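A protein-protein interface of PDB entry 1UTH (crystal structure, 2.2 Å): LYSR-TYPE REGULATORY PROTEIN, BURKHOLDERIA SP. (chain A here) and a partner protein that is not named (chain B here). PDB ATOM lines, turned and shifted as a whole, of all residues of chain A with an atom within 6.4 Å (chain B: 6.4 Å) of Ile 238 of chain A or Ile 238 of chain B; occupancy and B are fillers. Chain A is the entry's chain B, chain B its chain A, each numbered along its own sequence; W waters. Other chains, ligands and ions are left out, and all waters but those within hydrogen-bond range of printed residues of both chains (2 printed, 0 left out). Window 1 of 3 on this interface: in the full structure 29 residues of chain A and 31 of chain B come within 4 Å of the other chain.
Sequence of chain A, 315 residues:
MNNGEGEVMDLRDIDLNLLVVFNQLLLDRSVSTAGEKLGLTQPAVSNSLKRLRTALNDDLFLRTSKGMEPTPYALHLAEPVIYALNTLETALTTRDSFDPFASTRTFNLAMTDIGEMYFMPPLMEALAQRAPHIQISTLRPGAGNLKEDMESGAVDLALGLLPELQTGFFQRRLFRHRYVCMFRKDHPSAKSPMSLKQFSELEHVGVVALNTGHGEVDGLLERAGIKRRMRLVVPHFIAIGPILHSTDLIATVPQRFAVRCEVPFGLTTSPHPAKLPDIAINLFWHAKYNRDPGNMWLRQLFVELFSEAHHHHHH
Ile 238 of chain B touches Asp 113 of chain A. Glu 116 of chain A touches Ala 239 of chain B (O to CB, 3.7 Å). Met 117 of chain A touches Ile 238 of chain B (CE to O, 3.9 Å). Pro 242 of chain B touches Met 117 of chain A. Ile 238 of chain A touches Met 117 of chain B. Phe 237 of chain B touches Ile 238 of chain A (C to CD1, 3.97 Å). Ile 238 of chain B touches Ile 238 of chain A (N to CD1, 3.7 Å). CB of Ala 239 of chain A touches O of Glu 116 of chain B, 3.8 Å away. CE of Met 117 of chain B touches CG of Pro 242 of chain A, at 3.7 Å. Phe 265 of chain B touches Phe 265 of chain A.
Hydrophobic or aromatic side chains of chain B that line the printed part of chain A: Met 117, Ile 238, Ala 239, Pro 242 and Phe 265. Of the 15 printed residues of chain A, 7 touch a printed residue of chain B. Hydrophobic or aromatic side chains of chain A within 4 Å of the printed part of chain B: Met 117, Ile 238, Ala 239, Pro 242 and Phe 265. Among the printed residues, no Asp or Glu carboxylate lies within 4 Å of a Lys or Arg side-chain nitrogen of the other chain.
Water W1 lies within hydrogen-bond range of OE1 of Glu 116 of chain B, O of His 236 of chain A and N of Ala 239 of chain A. Water W2 lies within hydrogen-bond range of O of His 236 of chain B (2.7 Å), OE1 of Glu 116 of chain A (2.7 Å) and N of Ala 239 of chain B (2.8 Å).
The side-chain carboxylate of Asp 113 of chain B is in hydrogen-bond range of the backbone NH of Phe 237 of chain B. OE2 of Glu 116 of chain B is in salt-bridge range of NH1 of Arg 140 of chain B (2.6 Å). The side-chain carboxylate (OD2) of Asp 113 of chain A sits at hydrogen-bond distance from the backbone NH (N) of Phe 237 of chain A (3.0 Å). OE1 of Glu 116 of chain A is in salt-bridge range of NH2 of Arg 140 of chain A (2.6 Å).
Ile 114 of chain A touches none of the printed residues of chain B. Ile 238 of chain A touches just these residues of chain B: Asp 113 (3.8 Å), Met 117 (3.9 Å), Phe 237 (3.97 Å) and Ile 238 (3.7 Å). Of the printed residues of chain B, Ala 239 of chain A touches Glu 116 (3.8 Å) and Met 117 (3.8 Å). Printed residues of chain B within 4 Å of Phe 265 of chain A: Phe 265 (3.9 Å). Of the printed residues of chain A, Ala 239 of chain B touches Glu 116 (3.7 Å) and Met 117 (3.7 Å). Of the printed residues of chain A, Phe 265 of chain B touches Phe 265 (3.9 Å). The nearest residue of chain A that does not touch Ile 238 of chain B is Phe 237 of chain A (4.04 Å).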
ATOM      1  N   THR A 112     -24.902  20.768 -19.241  1.00  0.00           N
ATOM      2  CA  THR A 112     -25.440  19.801 -20.177  1.00  0.00           C
ATOM      3  C   THR A 112     -24.654  18.499 -20.119  1.00  0.00           C
ATOM      4  O   THR A 112     -23.635  18.410 -19.427  1.00  0.00           O
ATOM      5  CB  THR A 112     -25.363  20.305 -21.584  1.00  0.00           C
ATOM      6  OG1 THR A 112     -24.000  20.459 -21.961  1.00  0.00           O
ATOM      7  CG2 THR A 112     -25.939  21.722 -21.705  1.00  0.00           C
ATOM      8  N   ASP A 113     -25.110  17.510 -20.881  1.00  0.00           N
ATOM      9  CA  ASP A 113     -24.426  16.246 -20.900  1.00  0.00           C
ATOM     10  C   ASP A 113     -22.995  16.380 -21.429  1.00  0.00           C
ATOM     11  O   ASP A 113     -22.077  15.745 -20.876  1.00  0.00           O
ATOM     12  CB  ASP A 113     -25.299  15.105 -21.525  1.00  0.00           C
ATOM     13  CG  ASP A 113     -25.482  15.207 -23.033  1.00  0.00           C
ATOM     14  OD1 ASP A 113     -25.342  16.302 -23.619  1.00  0.00           O
ATOM     15  OD2 ASP A 113     -25.805  14.206 -23.709  1.00  0.00           O
ATOM     16  N   ILE A 114     -22.774  17.234 -22.427  1.00  0.00           N
ATOM     17  CA  ILE A 114     -21.425  17.480 -22.941  1.00  0.00           C
ATOM     18  C   ILE A 114     -20.579  18.220 -21.883  1.00  0.00           C
ATOM     19  O   ILE A 114     -19.376  17.979 -21.740  1.00  0.00           O
ATOM     20  CB  ILE A 114     -21.482  18.321 -24.255  1.00  0.00           C
ATOM     21  CG1 ILE A 114     -22.170  17.542 -25.366  1.00  0.00           C
ATOM     22  CG2 ILE A 114     -20.092  18.790 -24.684  1.00  0.00           C
ATOM     23  CD1 ILE A 114     -21.272  16.942 -26.390  1.00  0.00           C
ATOM     24  N   GLU A 116     -20.901  17.960 -18.614  1.00  0.00           N
ATOM     25  CA  GLU A 116     -20.611  17.036 -17.560  1.00  0.00           C
ATOM     26  C   GLU A 116     -19.423  16.217 -17.952  1.00  0.00           C
ATOM     27  O   GLU A 116     -18.496  16.112 -17.226  1.00  0.00           O
ATOM     28  CB  GLU A 116     -21.808  16.155 -17.312  1.00  0.00           C
ATOM     29  CG  GLU A 116     -21.889  15.676 -15.880  1.00  0.00           C
ATOM     30  CD  GLU A 116     -23.290  15.323 -15.517  1.00  0.00           C
ATOM     31  OE1 GLU A 116     -23.702  14.202 -15.925  1.00  0.00           O
ATOM     32  OE2 GLU A 116     -23.963  16.160 -14.859  1.00  0.00           O
ATOM     33  N   MET A 117     -19.423  15.728 -19.169  1.00  0.00           N
ATOM     34  CA  MET A 117     -18.346  14.913 -19.654  1.00  0.00           C
ATOM     35  C   MET A 117     -17.045  15.693 -19.854  1.00  0.00           C
ATOM     36  O   MET A 117     -15.955  15.100 -19.754  1.00  0.00           O
ATOM     37  CB  MET A 117     -18.807  14.167 -20.928  1.00  0.00           C
ATOM     38  CG  MET A 117     -17.997  14.368 -22.207  1.00  0.00           C
ATOM     39  SD  MET A 117     -18.342  13.033 -23.363  1.00  0.00           S
ATOM     40  CE  MET A 117     -17.858  11.553 -22.433  1.00  0.00           C
ATOM     41  N   ARG A 140     -29.123  18.969 -15.058  1.00  0.00           N
ATOM     42  CA  ARG A 140     -29.304  19.540 -16.380  1.00  0.00           C
ATOM     43  C   ARG A 140     -30.120  20.849 -16.262  1.00  0.00           C
ATOM     44  O   ARG A 140     -31.036  20.925 -15.463  1.00  0.00           O
ATOM     45  CB  ARG A 140     -30.048  18.554 -17.272  1.00  0.00           C
ATOM     46  CG  ARG A 140     -29.322  17.272 -17.559  1.00  0.00           C
ATOM     47  CD  ARG A 140     -28.178  17.389 -18.520  1.00  0.00           C
ATOM     48  NE  ARG A 140     -27.303  16.227 -18.450  1.00  0.00           N
ATOM     49  CZ  ARG A 140     -26.324  16.058 -17.552  1.00  0.00           C
ATOM     50  NH1 ARG A 140     -26.038  16.991 -16.638  1.00  0.00           N
ATOM     51  NH2 ARG A 140     -25.605  14.961 -17.594  1.00  0.00           N
ATOM     52  N   HIS A 236     -29.249  12.337 -27.229  1.00  0.00           N
ATOM     53  CA  HIS A 236     -28.162  12.828 -26.369  1.00  0.00           C
ATOM     54  C   HIS A 236     -26.858  12.175 -26.819  1.00  0.00           C
ATOM     55  O   HIS A 236     -26.861  11.377 -27.754  1.00  0.00           O
ATOM     56  CB  HIS A 236     -28.473  12.611 -24.879  1.00  0.00           C
ATOM     57  CG  HIS A 236     -29.705  13.314 -24.394  1.00  0.00           C
ATOM     58  ND1 HIS A 236     -29.965  14.646 -24.667  1.00  0.00           N
ATOM     59  CD2 HIS A 236     -30.748  12.877 -23.642  1.00  0.00           C
ATOM     60  CE1 HIS A 236     -31.125  14.986 -24.120  1.00  0.00           C
ATOM     61  NE2 HIS A 236     -31.629  13.930 -23.503  1.00  0.00           N
ATOM     62  N   PHE A 237     -25.737  12.579 -26.235  1.00  0.00           N
ATOM     63  CA  PHE A 237     -24.427  12.168 -26.732  1.00  0.00           C
ATOM     64  C   PHE A 237     -23.845  10.831 -26.222  1.00  0.00           C
ATOM     65  O   PHE A 237     -22.862  10.362 -26.771  1.00  0.00           O
ATOM     66  CB  PHE A 237     -23.416  13.294 -26.494  1.00  0.00           C
ATOM     67  CG  PHE A 237     -23.594  14.487 -27.448  1.00  0.00           C
ATOM     68  CD1 PHE A 237     -24.385  15.588 -27.083  1.00  0.00           C
ATOM     69  CD2 PHE A 237     -22.982  14.505 -28.671  1.00  0.00           C
ATOM     70  CE1 PHE A 237     -24.555  16.694 -27.947  1.00  0.00           C
ATOM     71  CE2 PHE A 237     -23.171  15.595 -29.550  1.00  0.00           C
ATOM     72  CZ  PHE A 237     -23.967  16.678 -29.174  1.00  0.00           C
ATOM     73  N   ILE A 238     -24.420  10.227 -25.188  1.00  0.00           N
ATOM     74  CA  ILE A 238     -23.785   9.068 -24.518  1.00  0.00           C
ATOM     75  C   ILE A 238     -23.282   7.918 -25.406  1.00  0.00           C
ATOM     76  O   ILE A 238     -22.112   7.551 -25.311  1.00  0.00           O
ATOM     77  CB  ILE A 238     -24.668   8.527 -23.357  1.00  0.00           C
ATOM     78  CG1 ILE A 238     -23.920   7.398 -22.608  1.00  0.00           C
ATOM     79  CG2 ILE A 238     -26.005   8.040 -23.834  1.00  0.00           C
ATOM     80  CD1 ILE A 238     -24.485   7.076 -21.245  1.00  0.00           C
ATOM     81  N   ALA A 239     -24.118   7.398 -26.306  1.00  0.00           N
ATOM     82  CA  ALA A 239     -23.747   6.264 -27.178  1.00  0.00           C
ATOM     83  C   ALA A 239     -22.878   6.579 -28.391  1.00  0.00           C
ATOM     84  O   ALA A 239     -22.494   5.656 -29.098  1.00  0.00           O
ATOM     85  CB  ALA A 239     -24.999   5.560 -27.658  1.00  0.00           C
ATOM     86  N   ILE A 240     -22.561   7.849 -28.653  1.00  0.00           N
ATOM     87  CA  ILE A 240     -21.880   8.209 -29.917  1.00  0.00           C
ATOM     88  C   ILE A 240     -20.522   7.539 -30.127  1.00  0.00           C
ATOM     89  O   ILE A 240     -20.260   6.998 -31.200  1.00  0.00           O
ATOM     90  CB  ILE A 240     -21.765   9.764 -30.065  1.00  0.00           C
ATOM     91  CG1 ILE A 240     -23.165  10.399 -30.292  1.00  0.00           C
ATOM     92  CG2 ILE A 240     -20.839  10.168 -31.172  1.00  0.00           C
ATOM     93  CD1 ILE A 240     -23.889   9.933 -31.560  1.00  0.00           C
ATOM     94  N   GLY A 241     -19.637   7.597 -29.146  1.00  0.00           N
ATOM     95  CA  GLY A 241     -18.353   6.892 -29.260  1.00  0.00           C
ATOM     96  C   GLY A 241     -18.458   5.425 -29.666  1.00  0.00           C
ATOM     97  O   GLY A 241     -17.952   5.018 -30.710  1.00  0.00           O
ATOM     98  N   PRO A 242     -19.149   4.624 -28.862  1.00  0.00           N
ATOM     99  CA  PRO A 242     -19.394   3.204 -29.197  1.00  0.00           C
ATOM    100  C   PRO A 242     -20.103   2.967 -30.550  1.00  0.00           C
ATOM    101  O   PRO A 242     -19.775   1.989 -31.244  1.00  0.00           O
ATOM    102  CB  PRO A 242     -20.260   2.700 -28.045  1.00  0.00           C
ATOM    103  CG  PRO A 242     -20.193   3.734 -26.971  1.00  0.00           C
ATOM    104  CD  PRO A 242     -19.691   5.004 -27.547  1.00  0.00           C
ATOM    105  N   PHE A 257     -15.982  17.279 -27.226  1.00  0.00           N
ATOM    106  CA  PHE A 257     -16.517  15.930 -27.091  1.00  0.00           C
ATOM    107  C   PHE A 257     -15.566  14.941 -27.738  1.00  0.00           C
ATOM    108  O   PHE A 257     -15.295  13.862 -27.197  1.00  0.00           O
ATOM    109  CB  PHE A 257     -17.873  15.855 -27.732  1.00  0.00           C
ATOM    110  CG  PHE A 257     -18.481  14.527 -27.660  1.00  0.00           C
ATOM    111  CD1 PHE A 257     -19.081  14.102 -26.502  1.00  0.00           C
ATOM    112  CD2 PHE A 257     -18.465  13.695 -28.746  1.00  0.00           C
ATOM    113  CE1 PHE A 257     -19.678  12.873 -26.439  1.00  0.00           C
ATOM    114  CE2 PHE A 257     -19.035  12.455 -28.672  1.00  0.00           C
ATOM    115  CZ  PHE A 257     -19.651  12.049 -27.527  1.00  0.00           C
ATOM    116  N   PHE A 265     -12.152   5.236 -27.990  1.00  0.00           N
ATOM    117  CA  PHE A 265     -13.001   4.543 -28.931  1.00  0.00           C
ATOM    118  C   PHE A 265     -12.373   4.336 -30.299  1.00  0.00           C
ATOM    119  O   PHE A 265     -13.027   3.844 -31.214  1.00  0.00           O
ATOM    120  CB  PHE A 265     -14.354   5.259 -29.007  1.00  0.00           C
ATOM    121  CG  PHE A 265     -15.179   5.109 -27.756  1.00  0.00           C
ATOM    122  CD1 PHE A 265     -15.356   6.168 -26.884  1.00  0.00           C
ATOM    123  CD2 PHE A 265     -15.759   3.914 -27.444  1.00  0.00           C
ATOM    124  CE1 PHE A 265     -16.079   6.023 -25.746  1.00  0.00           C
ATOM    125  CE2 PHE A 265     -16.507   3.773 -26.302  1.00  0.00           C
ATOM    126  CZ  PHE A 265     -16.656   4.834 -25.450  1.00  0.00           C
ATOM    127  N   THR B 112     -33.383   3.849 -22.249  1.00  0.00           N
ATOM    128  CA  THR B 112     -32.618   4.708 -21.344  1.00  0.00           C
ATOM    129  C   THR B 112     -31.291   4.987 -21.921  1.00  0.00           C
ATOM    130  O   THR B 112     -30.958   4.456 -22.956  1.00  0.00           O
ATOM    131  CB  THR B 112     -32.384   4.047 -19.998  1.00  0.00           C
ATOM    132  OG1 THR B 112     -31.584   2.876 -20.201  1.00  0.00           O
ATOM    133  CG2 THR B 112     -33.652   3.611 -19.429  1.00  0.00           C
ATOM    134  N   ASP B 113     -30.505   5.808 -21.239  1.00  0.00           N
ATOM    135  CA  ASP B 113     -29.141   6.066 -21.692  1.00  0.00           C
ATOM    136  C   ASP B 113     -28.266   4.813 -21.660  1.00  0.00           C
ATOM    137  O   ASP B 113     -27.524   4.595 -22.592  1.00  0.00           O
ATOM    138  CB  ASP B 113     -28.483   7.288 -20.991  1.00  0.00           C
ATOM    139  CG  ASP B 113     -28.349   7.120 -19.472  1.00  0.00           C
ATOM    140  OD1 ASP B 113     -27.638   7.981 -18.861  1.00  0.00           O
ATOM    141  OD2 ASP B 113     -28.923   6.203 -18.817  1.00  0.00           O
ATOM    142  N   ILE B 114     -28.381   3.959 -20.641  1.00  0.00           N
ATOM    143  CA  ILE B 114     -27.587   2.705 -20.632  1.00  0.00           C
ATOM    144  C   ILE B 114     -28.012   1.808 -21.815  1.00  0.00           C
ATOM    145  O   ILE B 114     -27.186   1.353 -22.588  1.00  0.00           O
ATOM    146  CB  ILE B 114     -27.796   1.884 -19.303  1.00  0.00           C
ATOM    147  CG1 ILE B 114     -27.386   2.678 -18.074  1.00  0.00           C
ATOM    148  CG2 ILE B 114     -27.104   0.460 -19.405  1.00  0.00           C
ATOM    149  CD1 ILE B 114     -25.955   2.708 -17.816  1.00  0.00           C
ATOM    150  N   GLU B 116     -29.299   2.697 -24.639  1.00  0.00           N
ATOM    151  CA  GLU B 116     -28.895   3.223 -25.909  1.00  0.00           C
ATOM    152  C   GLU B 116     -27.463   2.847 -26.141  1.00  0.00           C
ATOM    153  O   GLU B 116     -27.087   2.414 -27.206  1.00  0.00           O
ATOM    154  CB  GLU B 116     -29.093   4.728 -25.876  1.00  0.00           C
ATOM    155  CG  GLU B 116     -28.864   5.456 -27.176  1.00  0.00           C
ATOM    156  CD  GLU B 116     -29.460   6.850 -27.085  1.00  0.00           C
ATOM    157  OE1 GLU B 116     -28.690   7.829 -26.869  1.00  0.00           O
ATOM    158  OE2 GLU B 116     -30.713   6.930 -27.118  1.00  0.00           O
ATOM    159  N   MET B 117     -26.656   2.971 -25.108  1.00  0.00           N
ATOM    160  CA  MET B 117     -25.239   2.616 -25.196  1.00  0.00           C
ATOM    161  C   MET B 117     -25.006   1.117 -25.431  1.00  0.00           C
ATOM    162  O   MET B 117     -24.078   0.718 -26.153  1.00  0.00           O
ATOM    163  CB  MET B 117     -24.557   3.048 -23.904  1.00  0.00           C
ATOM    164  CG  MET B 117     -23.069   3.019 -23.965  1.00  0.00           C
ATOM    165  SD  MET B 117     -22.331   3.841 -22.519  1.00  0.00           S
ATOM    166  CE  MET B 117     -20.800   4.386 -23.382  1.00  0.00           C
ATOM    167  N   ARG B 140     -36.003   8.789 -24.958  1.00  0.00           N
ATOM    168  CA  ARG B 140     -35.971   8.301 -23.588  1.00  0.00           C
ATOM    169  C   ARG B 140     -37.395   8.049 -23.145  1.00  0.00           C
ATOM    170  O   ARG B 140     -38.267   8.745 -23.559  1.00  0.00           O
ATOM    171  CB  ARG B 140     -35.320   9.335 -22.667  1.00  0.00           C
ATOM    172  CG  ARG B 140     -33.823   9.572 -22.910  1.00  0.00           C
ATOM    173  CD  ARG B 140     -32.888   8.467 -22.381  1.00  0.00           C
ATOM    174  NE  ARG B 140     -31.567   8.609 -22.928  1.00  0.00           N
ATOM    175  CZ  ARG B 140     -31.205   8.219 -24.129  1.00  0.00           C
ATOM    176  NH1 ARG B 140     -32.054   7.588 -24.940  1.00  0.00           N
ATOM    177  NH2 ARG B 140     -29.965   8.454 -24.519  1.00  0.00           N
ATOM    178  N   HIS B 236     -27.119  11.340 -14.675  1.00  0.00           N
ATOM    179  CA  HIS B 236     -27.048  10.282 -15.670  1.00  0.00           C
ATOM    180  C   HIS B 236     -25.597   9.752 -15.871  1.00  0.00           C
ATOM    181  O   HIS B 236     -24.670  10.259 -15.246  1.00  0.00           O
ATOM    182  CB  HIS B 236     -27.593  10.832 -17.010  1.00  0.00           C
ATOM    183  CG  HIS B 236     -28.986  11.402 -16.916  1.00  0.00           C
ATOM    184  ND1 HIS B 236     -30.115  10.633 -17.073  1.00  0.00           N
ATOM    185  CD2 HIS B 236     -29.424  12.660 -16.657  1.00  0.00           C
ATOM    186  CE1 HIS B 236     -31.190  11.394 -16.917  1.00  0.00           C
ATOM    187  NE2 HIS B 236     -30.796  12.626 -16.664  1.00  0.00           N
ATOM    188  N   PHE B 237     -25.416   8.785 -16.770  1.00  0.00           N
ATOM    189  CA  PHE B 237     -24.227   7.943 -16.832  1.00  0.00           C
ATOM    190  C   PHE B 237     -23.106   8.435 -17.781  1.00  0.00           C
ATOM    191  O   PHE B 237     -21.980   7.917 -17.725  1.00  0.00           O
ATOM    192  CB  PHE B 237     -24.617   6.498 -17.207  1.00  0.00           C
ATOM    193  CG  PHE B 237     -25.290   5.741 -16.095  1.00  0.00           C
ATOM    194  CD1 PHE B 237     -26.661   5.766 -15.961  1.00  0.00           C
ATOM    195  CD2 PHE B 237     -24.543   5.005 -15.183  1.00  0.00           C
ATOM    196  CE1 PHE B 237     -27.304   5.082 -14.921  1.00  0.00           C
ATOM    197  CE2 PHE B 237     -25.159   4.313 -14.150  1.00  0.00           C
ATOM    198  CZ  PHE B 237     -26.552   4.376 -13.992  1.00  0.00           C
ATOM    199  N   ILE B 238     -23.393   9.442 -18.624  1.00  0.00           N
ATOM    200  CA  ILE B 238     -22.436   9.837 -19.663  1.00  0.00           C
ATOM    201  C   ILE B 238     -21.024  10.092 -19.202  1.00  0.00           C
ATOM    202  O   ILE B 238     -20.106   9.662 -19.874  1.00  0.00           O
ATOM    203  CB  ILE B 238     -22.940  11.066 -20.515  1.00  0.00           C
ATOM    204  CG1 ILE B 238     -22.001  11.310 -21.699  1.00  0.00           C
ATOM    205  CG2 ILE B 238     -23.088  12.311 -19.652  1.00  0.00           C
ATOM    206  CD1 ILE B 238     -22.411  12.497 -22.658  1.00  0.00           C
ATOM    207  N   ALA B 239     -20.812  10.808 -18.099  1.00  0.00           N
ATOM    208  CA  ALA B 239     -19.460  11.179 -17.706  1.00  0.00           C
ATOM    209  C   ALA B 239     -18.718  10.134 -16.817  1.00  0.00           C
ATOM    210  O   ALA B 239     -17.572  10.367 -16.446  1.00  0.00           O
ATOM    211  CB  ALA B 239     -19.480  12.546 -17.008  1.00  0.00           C
ATOM    212  N   ILE B 240     -19.362   9.016 -16.468  1.00  0.00           N
ATOM    213  CA  ILE B 240     -18.785   8.063 -15.504  1.00  0.00           C
ATOM    214  C   ILE B 240     -17.444   7.451 -15.921  1.00  0.00           C
ATOM    215  O   ILE B 240     -16.485   7.479 -15.149  1.00  0.00           O
ATOM    216  CB  ILE B 240     -19.805   6.971 -15.113  1.00  0.00           C
ATOM    217  CG1 ILE B 240     -21.027   7.569 -14.414  1.00  0.00           C
ATOM    218  CG2 ILE B 240     -19.186   5.903 -14.158  1.00  0.00           C
ATOM    219  CD1 ILE B 240     -20.770   8.339 -13.103  1.00  0.00           C
ATOM    220  N   GLY B 241     -17.358   6.887 -17.101  1.00  0.00           N
ATOM    221  CA  GLY B 241     -16.097   6.407 -17.623  1.00  0.00           C
ATOM    222  C   GLY B 241     -14.915   7.374 -17.490  1.00  0.00           C
ATOM    223  O   GLY B 241     -13.883   7.021 -16.941  1.00  0.00           O
ATOM    224  N   PRO B 242     -15.044   8.573 -18.050  1.00  0.00           N
ATOM    225  CA  PRO B 242     -14.012   9.615 -17.947  1.00  0.00           C
ATOM    226  C   PRO B 242     -13.746  10.048 -16.530  1.00  0.00           C
ATOM    227  O   PRO B 242     -12.605  10.352 -16.217  1.00  0.00           O
ATOM    228  CB  PRO B 242     -14.597  10.800 -18.771  1.00  0.00           C
ATOM    229  CG  PRO B 242     -15.602  10.205 -19.652  1.00  0.00           C
ATOM    230  CD  PRO B 242     -16.127   8.969 -18.965  1.00  0.00           C
ATOM    231  N   PHE B 257     -23.361  -1.561 -18.628  1.00  0.00           N
ATOM    232  CA  PHE B 257     -22.567  -0.337 -18.756  1.00  0.00           C
ATOM    233  C   PHE B 257     -21.055  -0.626 -18.700  1.00  0.00           C
ATOM    234  O   PHE B 257     -20.257  -0.070 -19.473  1.00  0.00           O
ATOM    235  CB  PHE B 257     -22.983   0.657 -17.693  1.00  0.00           C
ATOM    236  CG  PHE B 257     -22.266   1.975 -17.760  1.00  0.00           C
ATOM    237  CD1 PHE B 257     -22.593   2.921 -18.710  1.00  0.00           C
ATOM    238  CD2 PHE B 257     -21.251   2.266 -16.872  1.00  0.00           C
ATOM    239  CE1 PHE B 257     -21.931   4.122 -18.746  1.00  0.00           C
ATOM    240  CE2 PHE B 257     -20.579   3.494 -16.921  1.00  0.00           C
ATOM    241  CZ  PHE B 257     -20.922   4.406 -17.839  1.00  0.00           C
ATOM    242  N   PHE B 265     -11.969   3.073 -21.364  1.00  0.00           N
ATOM    243  CA  PHE B 265     -11.458   3.948 -20.297  1.00  0.00           C
ATOM    244  C   PHE B 265     -10.429   3.303 -19.324  1.00  0.00           C
ATOM    245  O   PHE B 265     -10.053   3.906 -18.334  1.00  0.00           O
ATOM    246  CB  PHE B 265     -12.643   4.565 -19.562  1.00  0.00           C
ATOM    247  CG  PHE B 265     -13.503   5.420 -20.444  1.00  0.00           C
ATOM    248  CD1 PHE B 265     -14.764   5.002 -20.821  1.00  0.00           C
ATOM    249  CD2 PHE B 265     -13.040   6.649 -20.912  1.00  0.00           C
ATOM    250  CE1 PHE B 265     -15.543   5.791 -21.650  1.00  0.00           C
ATOM    251  CE2 PHE B 265     -13.820   7.441 -21.734  1.00  0.00           C
ATOM    252  CZ  PHE B 265     -15.061   7.013 -22.109  1.00  0.00           C
HETATM  253  O   HOH W   1     -26.412   8.576 -27.630  1.00  0.00           O
HETATM  254  O   HOH W   2     -22.575  11.740 -16.091  1.00  0.00           O
